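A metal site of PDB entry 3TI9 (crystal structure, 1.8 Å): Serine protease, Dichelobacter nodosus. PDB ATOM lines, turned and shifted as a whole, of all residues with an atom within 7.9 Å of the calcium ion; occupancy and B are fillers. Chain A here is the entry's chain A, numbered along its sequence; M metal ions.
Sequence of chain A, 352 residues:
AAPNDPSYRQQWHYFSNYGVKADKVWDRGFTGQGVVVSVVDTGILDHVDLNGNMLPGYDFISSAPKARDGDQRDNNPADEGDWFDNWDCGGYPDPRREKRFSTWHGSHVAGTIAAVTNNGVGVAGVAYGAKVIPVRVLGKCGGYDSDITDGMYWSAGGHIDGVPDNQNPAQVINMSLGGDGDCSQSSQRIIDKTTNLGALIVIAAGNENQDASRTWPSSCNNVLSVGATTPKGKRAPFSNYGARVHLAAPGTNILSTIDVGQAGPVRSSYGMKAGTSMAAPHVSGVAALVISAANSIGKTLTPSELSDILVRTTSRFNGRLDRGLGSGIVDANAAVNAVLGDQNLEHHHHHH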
ATOM      1  N   PRO A   3       1.144 -21.987 -12.437  1.00  0.00           N
ATOM      2  CA  PRO A   3       2.393 -21.787 -13.169  1.00  0.00           C
ATOM      3  C   PRO A   3       3.422 -20.979 -12.373  1.00  0.00           C
ATOM      4  O   PRO A   3       3.044 -20.092 -11.597  1.00  0.00           O
ATOM      5  CB  PRO A   3       1.963 -21.016 -14.424  1.00  0.00           C
ATOM      6  CG  PRO A   3       0.534 -20.650 -14.222  1.00  0.00           C
ATOM      7  CD  PRO A   3      -0.034 -21.608 -13.237  1.00  0.00           C
ATOM      8  N   ASN A   4       4.706 -21.287 -12.550  1.00  0.00           N
ATOM      9  CA  ASN A   4       5.778 -20.645 -11.786  1.00  0.00           C
ATOM     10  C   ASN A   4       6.301 -19.334 -12.390  1.00  0.00           C
ATOM     11  O   ASN A   4       7.229 -18.717 -11.843  1.00  0.00           O
ATOM     12  CB  ASN A   4       6.935 -21.631 -11.498  1.00  0.00           C
ATOM     13  CG  ASN A   4       7.803 -21.928 -12.717  1.00  0.00           C
ATOM     14  OD1 ASN A   4       7.587 -21.395 -13.804  1.00  0.00           O
ATOM     15  ND2 ASN A   4       8.791 -22.793 -12.522  1.00  0.00           N
ATOM     16  N   ASP A   5       5.721 -18.919 -13.510  1.00  0.00           N
ATOM     17  CA  ASP A   5       6.125 -17.674 -14.162  1.00  0.00           C
ATOM     18  C   ASP A   5       5.910 -16.527 -13.162  1.00  0.00           C
ATOM     19  O   ASP A   5       4.820 -16.398 -12.609  1.00  0.00           O
ATOM     20  CB  ASP A   5       5.352 -17.487 -15.468  1.00  0.00           C
ATOM     21  CG  ASP A   5       5.319 -18.759 -16.294  1.00  0.00           C
ATOM     22  OD1 ASP A   5       6.119 -18.874 -17.245  1.00  0.00           O
ATOM     23  OD2 ASP A   5       4.519 -19.666 -15.966  1.00  0.00           O
ATOM     24  N   PRO A   6       6.965 -15.746 -12.886  1.00  0.00           N
ATOM     25  CA  PRO A   6       6.911 -14.756 -11.799  1.00  0.00           C
ATOM     26  C   PRO A   6       5.861 -13.649 -11.981  1.00  0.00           C
ATOM     27  O   PRO A   6       5.444 -13.052 -10.991  1.00  0.00           O
ATOM     28  CB  PRO A   6       8.326 -14.152 -11.789  1.00  0.00           C
ATOM     29  CG  PRO A   6       8.897 -14.476 -13.115  1.00  0.00           C
ATOM     30  CD  PRO A   6       8.290 -15.768 -13.540  1.00  0.00           C
ATOM     31  N   SER A   7       5.450 -13.401 -13.212  1.00  0.00           N
ATOM     32  CA  SER A   7       4.441 -12.375 -13.496  1.00  0.00           C
ATOM     33  C   SER A   7       3.031 -12.954 -13.683  1.00  0.00           C
ATOM     34  O   SER A   7       2.070 -12.200 -13.909  1.00  0.00           O
ATOM     35  CB  SER A   7       4.862 -11.513 -14.684  1.00  0.00           C
ATOM     36  OG  SER A   7       5.969 -10.686 -14.339  1.00  0.00           O
ATOM     37  N   TYR A   8       2.898 -14.274 -13.567  1.00  0.00           N
ATOM     38  CA  TYR A   8       1.582 -14.917 -13.648  1.00  0.00           C
ATOM     39  C   TYR A   8       0.616 -14.350 -12.612  1.00  0.00           C
ATOM     40  O   TYR A   8      -0.553 -14.132 -12.918  1.00  0.00           O
ATOM     41  CB  TYR A   8       1.683 -16.451 -13.486  1.00  0.00           C
ATOM     42  CG  TYR A   8       0.327 -17.101 -13.280  1.00  0.00           C
ATOM     43  CD1 TYR A   8      -0.607 -17.159 -14.320  1.00  0.00           C
ATOM     44  CD2 TYR A   8      -0.032 -17.624 -12.046  1.00  0.00           C
ATOM     45  CE1 TYR A   8      -1.860 -17.736 -14.143  1.00  0.00           C
ATOM     46  CE2 TYR A   8      -1.293 -18.216 -11.853  1.00  0.00           C
ATOM     47  CZ  TYR A   8      -2.198 -18.271 -12.910  1.00  0.00           C
ATOM     48  OH  TYR A   8      -3.431 -18.846 -12.733  1.00  0.00           O
ATOM     49  N   GLN A  11      -1.572 -11.651 -13.747  1.00  0.00           N
ATOM     50  CA  GLN A  11      -2.451 -11.937 -14.884  1.00  0.00           C
ATOM     51  C   GLN A  11      -3.852 -12.318 -14.397  1.00  0.00           C
ATOM     52  O   GLN A  11      -4.344 -13.424 -14.666  1.00  0.00           O
ATOM     53  CB  GLN A  11      -1.827 -12.985 -15.806  1.00  0.00           C
ATOM     54  CG  GLN A  11      -0.519 -12.503 -16.477  1.00  0.00           C
ATOM     55  CD  GLN A  11       0.096 -13.551 -17.399  1.00  0.00           C
ATOM     56  OE1 GLN A  11       0.576 -14.600 -16.949  1.00  0.00           O
ATOM     57  NE2 GLN A  11       0.069 -13.276 -18.707  1.00  0.00           N
ATOM     58  N   HIS A  47      11.691 -13.470 -28.619  1.00  0.00           N
ATOM     59  CA  HIS A  47      11.359 -13.269 -27.212  1.00  0.00           C
ATOM     60  C   HIS A  47      11.400 -14.608 -26.499  1.00  0.00           C
ATOM     61  O   HIS A  47      10.714 -15.560 -26.895  1.00  0.00           O
ATOM     62  CB  HIS A  47       9.961 -12.637 -27.088  1.00  0.00           C
ATOM     63  CG  HIS A  47       9.659 -12.041 -25.745  1.00  0.00           C
ATOM     64  ND1 HIS A  47       9.727 -12.759 -24.563  1.00  0.00           N
ATOM     65  CD2 HIS A  47       9.237 -10.798 -25.403  1.00  0.00           C
ATOM     66  CE1 HIS A  47       9.364 -11.987 -23.562  1.00  0.00           C
ATOM     67  NE2 HIS A  47       9.071 -10.794 -24.038  1.00  0.00           N
ATOM     68  N   VAL A  48      12.206 -14.683 -25.444  1.00  0.00           N
ATOM     69  CA  VAL A  48      12.403 -15.910 -24.656  1.00  0.00           C
ATOM     70  C   VAL A  48      11.071 -16.539 -24.232  1.00  0.00           C
ATOM     71  O   VAL A  48      10.971 -17.757 -24.090  1.00  0.00           O
ATOM     72  CB  VAL A  48      13.315 -15.672 -23.415  1.00  0.00           C
ATOM     73  CG1 VAL A  48      12.711 -14.616 -22.474  1.00  0.00           C
ATOM     74  CG2 VAL A  48      13.597 -16.983 -22.670  1.00  0.00           C
ATOM     75  N   ASP A  49      10.066 -15.703 -23.993  1.00  0.00           N
ATOM     76  CA  ASP A  49       8.763 -16.188 -23.542  1.00  0.00           C
ATOM     77  C   ASP A  49       7.770 -16.449 -24.679  1.00  0.00           C
ATOM     78  O   ASP A  49       6.579 -16.659 -24.425  1.00  0.00           O
ATOM     79  CB  ASP A  49       8.167 -15.246 -22.488  1.00  0.00           C
ATOM     80  CG  ASP A  49       7.790 -15.984 -21.225  1.00  0.00           C
ATOM     81  OD1 ASP A  49       8.349 -17.073 -20.987  1.00  0.00           O
ATOM     82  OD2 ASP A  49       6.932 -15.482 -20.460  1.00  0.00           O
ATOM     83  N   LEU A  50       8.276 -16.438 -25.912  1.00  0.00           N
ATOM     84  CA  LEU A  50       7.487 -16.744 -27.084  1.00  0.00           C
ATOM     85  C   LEU A  50       8.110 -17.842 -27.957  1.00  0.00           C
ATOM     86  O   LEU A  50       7.407 -18.745 -28.387  1.00  0.00           O
ATOM     87  CB  LEU A  50       7.262 -15.483 -27.934  1.00  0.00           C
ATOM     88  CG  LEU A  50       6.363 -14.378 -27.396  1.00  0.00           C
ATOM     89  CD1 LEU A  50       6.377 -13.152 -28.333  1.00  0.00           C
ATOM     90  CD2 LEU A  50       4.931 -14.865 -27.212  1.00  0.00           C
ATOM     91  N   ALA A 115       2.082 -17.795 -24.574  1.00  0.00           N
ATOM     92  CA  ALA A 115       3.375 -17.480 -23.962  1.00  0.00           C
ATOM     93  C   ALA A 115       3.920 -18.752 -23.305  1.00  0.00           C
ATOM     94  O   ALA A 115       3.146 -19.518 -22.709  1.00  0.00           O
ATOM     95  CB  ALA A 115       3.255 -16.360 -22.919  1.00  0.00           C
ATOM     96  N   VAL A 116       5.230 -18.980 -23.435  1.00  0.00           N
ATOM     97  CA  VAL A 116       5.873 -20.129 -22.799  1.00  0.00           C
ATOM     98  C   VAL A 116       5.630 -20.063 -21.300  1.00  0.00           C
ATOM     99  O   VAL A 116       5.958 -19.068 -20.644  1.00  0.00           O
ATOM    100  CB  VAL A 116       7.399 -20.222 -23.113  1.00  0.00           C
ATOM    101  CG1 VAL A 116       8.012 -21.467 -22.455  1.00  0.00           C
ATOM    102  CG2 VAL A 116       7.636 -20.239 -24.633  1.00  0.00           C
ATOM    103  N   THR A 117       5.030 -21.124 -20.760  1.00  0.00           N
ATOM    104  CA  THR A 117       4.579 -21.175 -19.360  1.00  0.00           C
ATOM    105  C   THR A 117       5.355 -22.257 -18.606  1.00  0.00           C
ATOM    106  O   THR A 117       5.843 -23.214 -19.213  1.00  0.00           O
ATOM    107  CB  THR A 117       3.055 -21.434 -19.332  1.00  0.00           C
ATOM    108  OG1 THR A 117       2.403 -20.411 -20.109  1.00  0.00           O
ATOM    109  CG2 THR A 117       2.489 -21.423 -17.909  1.00  0.00           C
ATOM    110  N   ASN A 118       5.484 -22.097 -17.289  1.00  0.00           N
ATOM    111  CA  ASN A 118       6.297 -22.985 -16.458  1.00  0.00           C
ATOM    112  C   ASN A 118       7.750 -23.047 -16.930  1.00  0.00           C
ATOM    113  O   ASN A 118       8.347 -24.129 -16.992  1.00  0.00           O
ATOM    114  CB  ASN A 118       5.667 -24.378 -16.350  1.00  0.00           C
ATOM    115  CG  ASN A 118       4.570 -24.448 -15.294  1.00  0.00           C
ATOM    116  OD1 ASN A 118       4.776 -23.753 -14.178  1.00  0.00           O
ATOM    117  ND2 ASN A 118       3.550 -25.113 -15.488  1.00  0.00           N
ATOM    118  N   ASN A 119       8.303 -21.885 -17.289  1.00  0.00           N
ATOM    119  CA  ASN A 119       9.719 -21.789 -17.637  1.00  0.00           C
ATOM    120  C   ASN A 119      10.493 -20.835 -16.708  1.00  0.00           C
ATOM    121  O   ASN A 119      11.625 -20.452 -17.006  1.00  0.00           O
ATOM    122  CB  ASN A 119       9.894 -21.428 -19.121  1.00  0.00           C
ATOM    123  CG  ASN A 119       9.450 -20.016 -19.451  1.00  0.00           C
ATOM    124  OD1 ASN A 119       8.661 -19.415 -18.725  1.00  0.00           O
ATOM    125  ND2 ASN A 119       9.956 -19.467 -20.554  1.00  0.00           N
ATOM    126  N   GLY A 120       9.874 -20.471 -15.592  1.00  0.00           N
ATOM    127  CA  GLY A 120      10.515 -19.645 -14.555  1.00  0.00           C
ATOM    128  C   GLY A 120      10.810 -18.207 -14.937  1.00  0.00           C
ATOM    129  O   GLY A 120      11.601 -17.526 -14.259  1.00  0.00           O
ATOM    130  N   VAL A 121      10.178 -17.726 -16.009  1.00  0.00           N
ATOM    131  CA  VAL A 121      10.430 -16.377 -16.544  1.00  0.00           C
ATOM    132  C   VAL A 121       9.137 -15.756 -17.080  1.00  0.00           C
ATOM    133  O   VAL A 121       8.267 -16.453 -17.618  1.00  0.00           O
ATOM    134  CB  VAL A 121      11.581 -16.366 -17.625  1.00  0.00           C
ATOM    135  CG1 VAL A 121      11.284 -17.302 -18.758  1.00  0.00           C
ATOM    136  CG2 VAL A 121      11.846 -14.958 -18.175  1.00  0.00           C
ATOM    137  N   GLY A 122       9.000 -14.442 -16.900  1.00  0.00           N
ATOM    138  CA  GLY A 122       7.895 -13.684 -17.456  1.00  0.00           C
ATOM    139  C   GLY A 122       6.504 -14.141 -17.076  1.00  0.00           C
ATOM    140  O   GLY A 122       6.164 -14.249 -15.897  1.00  0.00           O
ATOM    141  N   VAL A 123       5.703 -14.435 -18.106  1.00  0.00           N
ATOM    142  CA  VAL A 123       4.258 -14.596 -17.976  1.00  0.00           C
ATOM    143  C   VAL A 123       3.801 -15.995 -18.405  1.00  0.00           C
ATOM    144  O   VAL A 123       4.593 -16.827 -18.820  1.00  0.00           O
ATOM    145  CB  VAL A 123       3.498 -13.511 -18.788  1.00  0.00           C
ATOM    146  CG1 VAL A 123       3.725 -12.114 -18.179  1.00  0.00           C
ATOM    147  CG2 VAL A 123       3.899 -13.543 -20.277  1.00  0.00           C
ATOM    148  N   ALA A 124       2.490 -16.228 -18.313  1.00  0.00           N
ATOM    149  CA  ALA A 124       1.894 -17.462 -18.809  1.00  0.00           C
ATOM    150  C   ALA A 124       0.968 -17.148 -19.975  1.00  0.00           C
ATOM    151  O   ALA A 124       0.624 -15.984 -20.200  1.00  0.00           O
ATOM    152  CB  ALA A 124       1.127 -18.134 -17.702  1.00  0.00           C
ATOM    153  N   GLY A 125       0.596 -18.181 -20.735  1.00  0.00           N
ATOM    154  CA  GLY A 125      -0.397 -18.066 -21.819  1.00  0.00           C
ATOM    155  C   GLY A 125      -1.618 -18.919 -21.539  1.00  0.00           C
ATOM    156  O   GLY A 125      -1.507 -19.932 -20.836  1.00  0.00           O
ATOM    157  N   THR A 257       3.572 -10.368 -23.384  1.00  0.00           N
ATOM    158  CA  THR A 257       4.921 -10.233 -23.925  1.00  0.00           C
ATOM    159  C   THR A 257       5.028  -9.054 -24.883  1.00  0.00           C
ATOM    160  O   THR A 257       4.256  -8.950 -25.841  1.00  0.00           O
ATOM    161  CB  THR A 257       5.307 -11.517 -24.675  1.00  0.00           C
ATOM    162  OG1 THR A 257       4.192 -11.935 -25.478  1.00  0.00           O
ATOM    163  CG2 THR A 257       5.650 -12.634 -23.685  1.00  0.00           C
ATOM    164  N   TYR A 270       7.674  -7.253 -20.701  1.00  0.00           N
ATOM    165  CA  TYR A 270       6.272  -7.582 -20.447  1.00  0.00           C
ATOM    166  C   TYR A 270       5.574  -6.293 -20.114  1.00  0.00           C
ATOM    167  O   TYR A 270       6.161  -5.402 -19.492  1.00  0.00           O
ATOM    168  CB  TYR A 270       6.165  -8.620 -19.318  1.00  0.00           C
ATOM    169  CG  TYR A 270       7.139  -9.758 -19.543  1.00  0.00           C
ATOM    170  CD1 TYR A 270       6.796 -10.830 -20.361  1.00  0.00           C
ATOM    171  CD2 TYR A 270       8.422  -9.727 -19.002  1.00  0.00           C
ATOM    172  CE1 TYR A 270       7.698 -11.860 -20.607  1.00  0.00           C
ATOM    173  CE2 TYR A 270       9.331 -10.735 -19.257  1.00  0.00           C
ATOM    174  CZ  TYR A 270       8.969 -11.795 -20.059  1.00  0.00           C
ATOM    175  OH  TYR A 270       9.860 -12.805 -20.298  1.00  0.00           O
HETATM  176 CA    CA M   1       6.850 -17.686 -19.041  1.00  0.00          CA
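The calcium ion is bound by OD1 of Asp 5 (2.3 Å), O of Val 116 (2.3 Å), O of Val 121 (2.4 Å), O of Val 123 (2.4 Å), OD1 of Asn 119 (2.5 Å), OD1 of Asp 49 (2.5 Å) and OD2 of Asp 49 (2.6 Å).
The calcium ion has seven donor atoms within binding distance.
The side-chain carboxylate (OD2) of Asp 5 is in hydrogen-bond range of the backbone NH (N) of Asn 118.
ND1 of His 47 is in hydrogen-bond range of N of Asp 49, 3.0 Å away.
Of the 24 residues printed, 6 come within 4 Å of the calcium ion.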
